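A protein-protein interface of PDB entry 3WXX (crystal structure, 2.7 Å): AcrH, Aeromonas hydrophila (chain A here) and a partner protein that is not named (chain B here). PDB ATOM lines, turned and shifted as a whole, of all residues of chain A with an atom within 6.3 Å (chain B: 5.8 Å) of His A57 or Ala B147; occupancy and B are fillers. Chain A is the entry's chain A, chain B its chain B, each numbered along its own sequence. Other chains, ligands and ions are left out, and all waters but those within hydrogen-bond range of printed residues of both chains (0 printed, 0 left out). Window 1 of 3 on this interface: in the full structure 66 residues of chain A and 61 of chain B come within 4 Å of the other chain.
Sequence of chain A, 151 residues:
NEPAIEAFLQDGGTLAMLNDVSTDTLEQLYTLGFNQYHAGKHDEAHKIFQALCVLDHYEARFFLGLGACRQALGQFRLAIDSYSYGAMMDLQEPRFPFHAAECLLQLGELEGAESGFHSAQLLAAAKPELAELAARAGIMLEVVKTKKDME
A ring nitrogen (NE2) of His A57 is in hydrogen-bond range of the backbone NH (N) of Ala B144.
The side-chain sulfur (SG) of Cys A53 is in hydrogen-bond range of the backbone carbonyl oxygen (O) of Phe A62 (3.4 Å). N of Phe A63 lies close to SG of Cys A53 (3.8 Å). N of Tyr A58 lies within hydrogen-bond range of OD1 of Asp A56 (3.0 Å). NE2 of His A57 lies within hydrogen-bond range of OH of Tyr A58, at 3.2 Å. The side-chain hydroxyl (OH) of Tyr A85 sits at hydrogen-bond distance from the backbone carbonyl oxygen (O) of His A57 (2.5 Å).
Gly B140 touches Leu A9 (CA to O, 3.3 Å). Leu A9 touches Ala B144. CB of Cys A53 touches CG2 of Val B151, at 3.4 Å. CG2 of Val A54 touches CG1 of Val B151, 3.9 Å away. His A57 touches Ala B143. His A57 touches Ala B147. Tyr A58 touches Gly B140 (OH to CA, 3.3 Å). CE1 of Tyr A85 touches CG1 of Val B131, at 3.8 Å. Tyr A85 touches Ala B143. Ile B150 touches Tyr A85.
Of the printed residues of chain B, Leu A9 touches Gly B140 (3.3 Å) and Ala B144 (3.9 Å). Leu A55 touches none of the printed residues of chain B. Printed residues of chain B within 4 Å of His A57: Gly B140 (3.8 Å), Ala B143 (3.7 Å), Ala B144 (3.5 Å) and Ala B147 (3.6 Å). Of the printed residues of chain B, Tyr A58 touches Gly B140 (3.3 Å) and Ala B143 (3.9 Å). Printed residues of chain B within 4 Å of Tyr A85: Val B131 (3.8 Å), Ala B143 (3.6 Å) and Ile B150 (3.6 Å). Gly B142 touches none of the printed residues of chain A. Of chain A, only His A57 (3.6 Å) comes within 4 Å of Ala B147. The nearest residue of chain A that does not touch Ala B147 is Phe A63 (4.02 Å).
Hydrophobic or aromatic side chains of chain A within 4 Å of the printed part of chain B: Leu A9, Val A54, His A57, Tyr A58 and Tyr A85. Hydrophobic or aromatic side chains of chain B within 4 Å of the printed part of chain A: Val B131, Ala B143, Ala B144, Ala B147, Ile B150 and Val B151. Among the printed residues, 13 pairs touch across the chains. Among the printed residues, no Asp or Glu carboxylate lies within 4 Å of a Lys or Arg side-chain nitrogen of the other chain.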
ATOM      1  N   LEU A   9     -21.848 -12.367 -15.608  1.00  0.00           N
ATOM      2  CA  LEU A   9     -21.788 -12.595 -17.030  1.00  0.00           C
ATOM      3  C   LEU A   9     -22.135 -14.045 -17.309  1.00  0.00           C
ATOM      4  O   LEU A   9     -22.897 -14.350 -18.239  1.00  0.00           O
ATOM      5  CB  LEU A   9     -20.374 -12.266 -17.555  1.00  0.00           C
ATOM      6  CG  LEU A   9     -20.161 -12.360 -19.067  1.00  0.00           C
ATOM      7  CD1 LEU A   9     -20.979 -11.313 -19.789  1.00  0.00           C
ATOM      8  CD2 LEU A   9     -18.712 -12.173 -19.416  1.00  0.00           C
ATOM      9  N   GLY A  12     -25.728 -15.156 -16.882  1.00  0.00           N
ATOM     10  CA  GLY A  12     -26.586 -14.757 -17.979  1.00  0.00           C
ATOM     11  C   GLY A  12     -26.911 -13.288 -17.962  1.00  0.00           C
ATOM     12  O   GLY A  12     -27.762 -12.832 -18.719  1.00  0.00           O
ATOM     13  N   GLY A  13     -26.201 -12.525 -17.143  1.00  0.00           N
ATOM     14  CA  GLY A  13     -26.274 -11.098 -17.282  1.00  0.00           C
ATOM     15  C   GLY A  13     -25.671 -10.612 -18.604  1.00  0.00           C
ATOM     16  O   GLY A  13     -24.808 -11.285 -19.233  1.00  0.00           O
ATOM     17  N   THR A  14     -26.132  -9.426 -18.990  1.00  0.00           N
ATOM     18  CA  THR A  14     -25.786  -8.788 -20.232  1.00  0.00           C
ATOM     19  C   THR A  14     -25.226  -7.413 -20.003  1.00  0.00           C
ATOM     20  O   THR A  14     -25.402  -6.842 -18.952  1.00  0.00           O
ATOM     21  CB  THR A  14     -27.017  -8.616 -21.088  1.00  0.00           C
ATOM     22  OG1 THR A  14     -27.743  -7.495 -20.610  1.00  0.00           O
ATOM     23  CG2 THR A  14     -27.888  -9.848 -20.992  1.00  0.00           C
ATOM     24  N   LEU A  15     -24.599  -6.878 -21.030  1.00  0.00           N
ATOM     25  CA  LEU A  15     -24.084  -5.513 -21.018  1.00  0.00           C
ATOM     26  C   LEU A  15     -25.184  -4.459 -20.815  1.00  0.00           C
ATOM     27  O   LEU A  15     -24.946  -3.429 -20.215  1.00  0.00           O
ATOM     28  CB  LEU A  15     -23.358  -5.223 -22.332  1.00  0.00           C
ATOM     29  CG  LEU A  15     -22.630  -3.903 -22.494  1.00  0.00           C
ATOM     30  CD1 LEU A  15     -21.449  -3.814 -21.574  1.00  0.00           C
ATOM     31  CD2 LEU A  15     -22.155  -3.777 -23.929  1.00  0.00           C
ATOM     32  N   LEU A  52     -26.863  -3.816 -30.780  1.00  0.00           N
ATOM     33  CA  LEU A  52     -27.905  -4.550 -30.049  1.00  0.00           C
ATOM     34  C   LEU A  52     -27.428  -5.959 -29.599  1.00  0.00           C
ATOM     35  O   LEU A  52     -27.626  -6.345 -28.448  1.00  0.00           O
ATOM     36  CB  LEU A  52     -29.151  -4.684 -30.926  1.00  0.00           C
ATOM     37  CG  LEU A  52     -29.872  -3.388 -31.254  1.00  0.00           C
ATOM     38  CD1 LEU A  52     -30.896  -3.564 -32.351  1.00  0.00           C
ATOM     39  CD2 LEU A  52     -30.530  -2.884 -30.009  1.00  0.00           C
ATOM     40  N   CYS A  53     -26.808  -6.701 -30.518  1.00  0.00           N
ATOM     41  CA  CYS A  53     -26.338  -8.021 -30.219  1.00  0.00           C
ATOM     42  C   CYS A  53     -25.339  -8.020 -29.103  1.00  0.00           C
ATOM     43  O   CYS A  53     -25.253  -8.951 -28.325  1.00  0.00           O
ATOM     44  CB  CYS A  53     -25.737  -8.668 -31.455  1.00  0.00           C
ATOM     45  SG  CYS A  53     -26.962  -9.139 -32.669  1.00  0.00           S
ATOM     46  N   VAL A  54     -24.551  -6.971 -29.024  1.00  0.00           N
ATOM     47  CA  VAL A  54     -23.580  -6.830 -27.928  1.00  0.00           C
ATOM     48  C   VAL A  54     -24.287  -6.417 -26.619  1.00  0.00           C
ATOM     49  O   VAL A  54     -23.909  -6.866 -25.563  1.00  0.00           O
ATOM     50  CB  VAL A  54     -22.478  -5.830 -28.330  1.00  0.00           C
ATOM     51  CG1 VAL A  54     -21.718  -5.344 -27.120  1.00  0.00           C
ATOM     52  CG2 VAL A  54     -21.529  -6.460 -29.336  1.00  0.00           C
ATOM     53  N   LEU A  55     -25.300  -5.562 -26.714  1.00  0.00           N
ATOM     54  CA  LEU A  55     -26.054  -5.094 -25.537  1.00  0.00           C
ATOM     55  C   LEU A  55     -26.874  -6.186 -24.894  1.00  0.00           C
ATOM     56  O   LEU A  55     -26.943  -6.259 -23.677  1.00  0.00           O
ATOM     57  CB  LEU A  55     -26.957  -3.908 -25.905  1.00  0.00           C
ATOM     58  CG  LEU A  55     -26.159  -2.623 -26.150  1.00  0.00           C
ATOM     59  CD1 LEU A  55     -26.954  -1.593 -26.915  1.00  0.00           C
ATOM     60  CD2 LEU A  55     -25.667  -2.052 -24.835  1.00  0.00           C
ATOM     61  N   ASP A  56     -27.477  -7.044 -25.703  1.00  0.00           N
ATOM     62  CA  ASP A  56     -28.156  -8.215 -25.174  1.00  0.00           C
ATOM     63  C   ASP A  56     -27.845  -9.408 -26.096  1.00  0.00           C
ATOM     64  O   ASP A  56     -28.423  -9.540 -27.158  1.00  0.00           O
ATOM     65  CB  ASP A  56     -29.655  -7.959 -25.055  1.00  0.00           C
ATOM     66  CG  ASP A  56     -30.445  -9.142 -24.433  1.00  0.00           C
ATOM     67  OD1 ASP A  56     -29.991 -10.304 -24.422  1.00  0.00           O
ATOM     68  OD2 ASP A  56     -31.586  -8.895 -23.997  1.00  0.00           O
ATOM     69  N   HIS A  57     -26.965 -10.293 -25.655  1.00  0.00           N
ATOM     70  CA  HIS A  57     -26.447 -11.302 -26.529  1.00  0.00           C
ATOM     71  C   HIS A  57     -27.246 -12.584 -26.420  1.00  0.00           C
ATOM     72  O   HIS A  57     -26.773 -13.660 -26.826  1.00  0.00           O
ATOM     73  CB  HIS A  57     -24.938 -11.517 -26.288  1.00  0.00           C
ATOM     74  CG  HIS A  57     -24.587 -12.055 -24.924  1.00  0.00           C
ATOM     75  ND1 HIS A  57     -24.356 -11.247 -23.835  1.00  0.00           N
ATOM     76  CD2 HIS A  57     -24.370 -13.318 -24.492  1.00  0.00           C
ATOM     77  CE1 HIS A  57     -24.017 -11.981 -22.791  1.00  0.00           C
ATOM     78  NE2 HIS A  57     -24.000 -13.242 -23.167  1.00  0.00           N
ATOM     79  N   TYR A  58     -28.445 -12.449 -25.862  1.00  0.00           N
ATOM     80  CA  TYR A  58     -29.435 -13.550 -25.814  1.00  0.00           C
ATOM     81  C   TYR A  58     -30.702 -13.305 -26.652  1.00  0.00           C
ATOM     82  O   TYR A  58     -31.443 -14.236 -26.836  1.00  0.00           O
ATOM     83  CB  TYR A  58     -29.801 -13.926 -24.371  1.00  0.00           C
ATOM     84  CG  TYR A  58     -28.609 -14.322 -23.498  1.00  0.00           C
ATOM     85  CD1 TYR A  58     -28.078 -15.625 -23.508  1.00  0.00           C
ATOM     86  CD2 TYR A  58     -28.029 -13.393 -22.641  1.00  0.00           C
ATOM     87  CE1 TYR A  58     -26.974 -15.965 -22.695  1.00  0.00           C
ATOM     88  CE2 TYR A  58     -26.959 -13.711 -21.828  1.00  0.00           C
ATOM     89  CZ  TYR A  58     -26.417 -14.992 -21.848  1.00  0.00           C
ATOM     90  OH  TYR A  58     -25.332 -15.211 -21.017  1.00  0.00           O
ATOM     91  N   GLU A  59     -30.904 -12.103 -27.211  1.00  0.00           N
ATOM     92  CA  GLU A  59     -32.065 -11.819 -28.101  1.00  0.00           C
ATOM     93  C   GLU A  59     -31.902 -12.350 -29.514  1.00  0.00           C
ATOM     94  O   GLU A  59     -31.198 -11.736 -30.324  1.00  0.00           O
ATOM     95  CB  GLU A  59     -32.276 -10.318 -28.300  1.00  0.00           C
ATOM     96  CG  GLU A  59     -33.142  -9.631 -27.294  1.00  0.00           C
ATOM     97  CD  GLU A  59     -34.525 -10.186 -27.222  1.00  0.00           C
ATOM     98  OE1 GLU A  59     -35.349  -9.785 -28.039  1.00  0.00           O
ATOM     99  OE2 GLU A  59     -34.788 -11.000 -26.325  1.00  0.00           O
ATOM    100  N   PHE A  62     -32.344  -9.683 -32.463  1.00  0.00           N
ATOM    101  CA  PHE A  62     -31.132  -8.886 -32.827  1.00  0.00           C
ATOM    102  C   PHE A  62     -30.215  -9.694 -33.755  1.00  0.00           C
ATOM    103  O   PHE A  62     -29.641  -9.150 -34.685  1.00  0.00           O
ATOM    104  CB  PHE A  62     -30.346  -8.426 -31.590  1.00  0.00           C
ATOM    105  CG  PHE A  62     -31.170  -7.627 -30.593  1.00  0.00           C
ATOM    106  CD1 PHE A  62     -32.449  -7.183 -30.904  1.00  0.00           C
ATOM    107  CD2 PHE A  62     -30.653  -7.319 -29.352  1.00  0.00           C
ATOM    108  CE1 PHE A  62     -33.180  -6.437 -29.996  1.00  0.00           C
ATOM    109  CE2 PHE A  62     -31.393  -6.582 -28.426  1.00  0.00           C
ATOM    110  CZ  PHE A  62     -32.653  -6.131 -28.752  1.00  0.00           C
ATOM    111  N   PHE A  63     -30.111 -11.004 -33.529  1.00  0.00           N
ATOM    112  CA  PHE A  63     -29.357 -11.870 -34.436  1.00  0.00           C
ATOM    113  C   PHE A  63     -30.054 -12.121 -35.737  1.00  0.00           C
ATOM    114  O   PHE A  63     -29.422 -12.236 -36.760  1.00  0.00           O
ATOM    115  CB  PHE A  63     -28.932 -13.152 -33.718  1.00  0.00           C
ATOM    116  CG  PHE A  63     -27.947 -12.859 -32.628  1.00  0.00           C
ATOM    117  CD1 PHE A  63     -26.563 -12.683 -32.941  1.00  0.00           C
ATOM    118  CD2 PHE A  63     -28.374 -12.589 -31.357  1.00  0.00           C
ATOM    119  CE1 PHE A  63     -25.652 -12.332 -31.958  1.00  0.00           C
ATOM    120  CE2 PHE A  63     -27.447 -12.253 -30.363  1.00  0.00           C
ATOM    121  CZ  PHE A  63     -26.085 -12.136 -30.662  1.00  0.00           C
ATOM    122  N   TYR A  85     -26.224 -18.543 -34.541  1.00  0.00           N
ATOM    123  CA  TYR A  85     -26.335 -18.175 -33.129  1.00  0.00           C
ATOM    124  C   TYR A  85     -27.777 -17.808 -32.770  1.00  0.00           C
ATOM    125  O   TYR A  85     -28.256 -18.187 -31.750  1.00  0.00           O
ATOM    126  CB  TYR A  85     -25.387 -17.037 -32.743  1.00  0.00           C
ATOM    127  CG  TYR A  85     -25.411 -16.670 -31.272  1.00  0.00           C
ATOM    128  CD1 TYR A  85     -24.628 -17.337 -30.376  1.00  0.00           C
ATOM    129  CD2 TYR A  85     -26.205 -15.659 -30.798  1.00  0.00           C
ATOM    130  CE1 TYR A  85     -24.612 -17.015 -29.026  1.00  0.00           C
ATOM    131  CE2 TYR A  85     -26.237 -15.345 -29.443  1.00  0.00           C
ATOM    132  CZ  TYR A  85     -25.413 -16.010 -28.549  1.00  0.00           C
ATOM    133  OH  TYR A  85     -25.400 -15.729 -27.145  1.00  0.00           O
ATOM    134  N   MET A  89     -30.588 -19.483 -29.791  1.00  0.00           N
ATOM    135  CA  MET A  89     -31.317 -18.710 -28.785  1.00  0.00           C
ATOM    136  C   MET A  89     -32.810 -18.808 -28.953  1.00  0.00           C
ATOM    137  O   MET A  89     -33.568 -18.314 -28.125  1.00  0.00           O
ATOM    138  CB  MET A  89     -30.945 -17.219 -28.861  1.00  0.00           C
ATOM    139  CG  MET A  89     -29.466 -16.945 -28.631  1.00  0.00           C
ATOM    140  SD  MET A  89     -28.976 -17.431 -26.778  1.00  0.00           S
ATOM    141  CE  MET A  89     -28.215 -19.229 -26.998  1.00  0.00           C
ATOM    142  N   VAL B 131     -19.317 -22.089 -30.523  1.00  0.00           N
ATOM    143  CA  VAL B 131     -20.031 -21.297 -29.515  1.00  0.00           C
ATOM    144  C   VAL B 131     -20.927 -22.207 -28.657  1.00  0.00           C
ATOM    145  O   VAL B 131     -21.010 -22.037 -27.450  1.00  0.00           O
ATOM    146  CB  VAL B 131     -20.829 -20.133 -30.157  1.00  0.00           C
ATOM    147  CG1 VAL B 131     -21.554 -19.331 -29.106  1.00  0.00           C
ATOM    148  CG2 VAL B 131     -19.891 -19.214 -30.928  1.00  0.00           C
ATOM    149  N   GLY B 140     -22.704 -18.494 -19.600  1.00  0.00           N
ATOM    150  CA  GLY B 140     -22.841 -17.113 -20.054  1.00  0.00           C
ATOM    151  C   GLY B 140     -21.561 -16.444 -20.538  1.00  0.00           C
ATOM    152  O   GLY B 140     -21.619 -15.547 -21.392  1.00  0.00           O
ATOM    153  N   GLY B 142     -19.180 -18.141 -22.148  1.00  0.00           N
ATOM    154  CA  GLY B 142     -19.115 -18.726 -23.499  1.00  0.00           C
ATOM    155  C   GLY B 142     -20.006 -18.025 -24.489  1.00  0.00           C
ATOM    156  O   GLY B 142     -19.600 -17.688 -25.593  1.00  0.00           O
ATOM    157  N   ALA B 143     -21.236 -17.780 -24.091  1.00  0.00           N
ATOM    158  CA  ALA B 143     -22.156 -17.084 -24.976  1.00  0.00           C
ATOM    159  C   ALA B 143     -21.611 -15.703 -25.293  1.00  0.00           C
ATOM    160  O   ALA B 143     -21.608 -15.293 -26.442  1.00  0.00           O
ATOM    161  CB  ALA B 143     -23.525 -16.949 -24.343  1.00  0.00           C
ATOM    162  N   ALA B 144     -21.199 -14.989 -24.249  1.00  0.00           N
ATOM    163  CA  ALA B 144     -20.644 -13.658 -24.416  1.00  0.00           C
ATOM    164  C   ALA B 144     -19.536 -13.616 -25.463  1.00  0.00           C
ATOM    165  O   ALA B 144     -19.684 -12.990 -26.489  1.00  0.00           O
ATOM    166  CB  ALA B 144     -20.098 -13.151 -23.104  1.00  0.00           C
ATOM    167  N   VAL B 145     -18.456 -14.339 -25.240  1.00  0.00           N
ATOM    168  CA  VAL B 145     -17.376 -14.285 -26.201  1.00  0.00           C
ATOM    169  C   VAL B 145     -17.846 -14.775 -27.574  1.00  0.00           C
ATOM    170  O   VAL B 145     -17.343 -14.309 -28.615  1.00  0.00           O
ATOM    171  CB  VAL B 145     -16.131 -15.075 -25.729  1.00  0.00           C
ATOM    172  CG1 VAL B 145     -16.420 -16.569 -25.704  1.00  0.00           C
ATOM    173  CG2 VAL B 145     -14.919 -14.768 -26.598  1.00  0.00           C
ATOM    174  N   GLY B 146     -18.768 -15.745 -27.585  1.00  0.00           N
ATOM    175  CA  GLY B 146     -19.270 -16.295 -28.860  1.00  0.00           C
ATOM    176  C   GLY B 146     -20.006 -15.253 -29.641  1.00  0.00           C
ATOM    177  O   GLY B 146     -19.811 -15.086 -30.847  1.00  0.00           O
ATOM    178  N   ALA B 147     -20.834 -14.501 -28.958  1.00  0.00           N
ATOM    179  CA  ALA B 147     -21.564 -13.460 -29.644  1.00  0.00           C
ATOM    180  C   ALA B 147     -20.610 -12.372 -30.136  1.00  0.00           C
ATOM    181  O   ALA B 147     -20.800 -11.833 -31.219  1.00  0.00           O
ATOM    182  CB  ALA B 147     -22.627 -12.872 -28.740  1.00  0.00           C
ATOM    183  N   MET B 148     -19.606 -12.051 -29.326  1.00  0.00           N
ATOM    184  CA  MET B 148     -18.568 -11.123 -29.724  1.00  0.00           C
ATOM    185  C   MET B 148     -17.918 -11.543 -31.006  1.00  0.00           C
ATOM    186  O   MET B 148     -17.847 -10.768 -31.939  1.00  0.00           O
ATOM    187  CB  MET B 148     -17.451 -11.028 -28.692  1.00  0.00           C
ATOM    188  CG  MET B 148     -17.899 -10.416 -27.357  1.00  0.00           C
ATOM    189  SD  MET B 148     -17.925  -8.495 -27.522  1.00  0.00           S
ATOM    190  CE  MET B 148     -17.794  -8.310 -25.589  1.00  0.00           C
ATOM    191  N   MET B 149     -17.471 -12.776 -31.108  1.00  0.00           N
ATOM    192  CA  MET B 149     -16.909 -13.191 -32.354  1.00  0.00           C
ATOM    193  C   MET B 149     -17.824 -13.006 -33.553  1.00  0.00           C
ATOM    194  O   MET B 149     -17.370 -12.620 -34.659  1.00  0.00           O
ATOM    195  CB  MET B 149     -16.627 -14.652 -32.264  1.00  0.00           C
ATOM    196  CG  MET B 149     -15.475 -14.840 -31.321  1.00  0.00           C
ATOM    197  SD  MET B 149     -15.315 -16.764 -31.050  1.00  0.00           S
ATOM    198  CE  MET B 149     -15.392 -17.278 -32.954  1.00  0.00           C
ATOM    199  N   ILE B 150     -19.117 -13.321 -33.365  1.00  0.00           N
ATOM    200  CA  ILE B 150     -20.055 -13.298 -34.469  1.00  0.00           C
ATOM    201  C   ILE B 150     -20.440 -11.885 -34.835  1.00  0.00           C
ATOM    202  O   ILE B 150     -20.524 -11.552 -36.012  1.00  0.00           O
ATOM    203  CB  ILE B 150     -21.279 -14.122 -34.138  1.00  0.00           C
ATOM    204  CG1 ILE B 150     -20.907 -15.607 -34.248  1.00  0.00           C
ATOM    205  CG2 ILE B 150     -22.430 -13.762 -35.065  1.00  0.00           C
ATOM    206  CD1 ILE B 150     -22.015 -16.529 -33.804  1.00  0.00           C
ATOM    207  N   VAL B 151     -20.632 -11.037 -33.832  1.00  0.00           N
ATOM    208  CA  VAL B 151     -20.842  -9.623 -34.115  1.00  0.00           C
ATOM    209  C   VAL B 151     -19.734  -8.996 -34.978  1.00  0.00           C
ATOM    210  O   VAL B 151     -20.044  -8.176 -35.837  1.00  0.00           O
ATOM    211  CB  VAL B 151     -21.066  -8.804 -32.836  1.00  0.00           C
ATOM    212  CG1 VAL B 151     -20.813  -7.337 -33.076  1.00  0.00           C
ATOM    213  CG2 VAL B 151     -22.496  -8.973 -32.395  1.00  0.00           C
ATOM    214  N   GLY B 152     -18.465  -9.369 -34.782  1.00  0.00           N
ATOM    215  CA  GLY B 152     -17.403  -8.906 -35.689  1.00  0.00           C
ATOM    216  C   GLY B 152     -16.644  -7.684 -35.204  1.00  0.00           C
ATOM    217  O   GLY B 152     -15.414  -7.701 -35.110  1.00  0.00           O
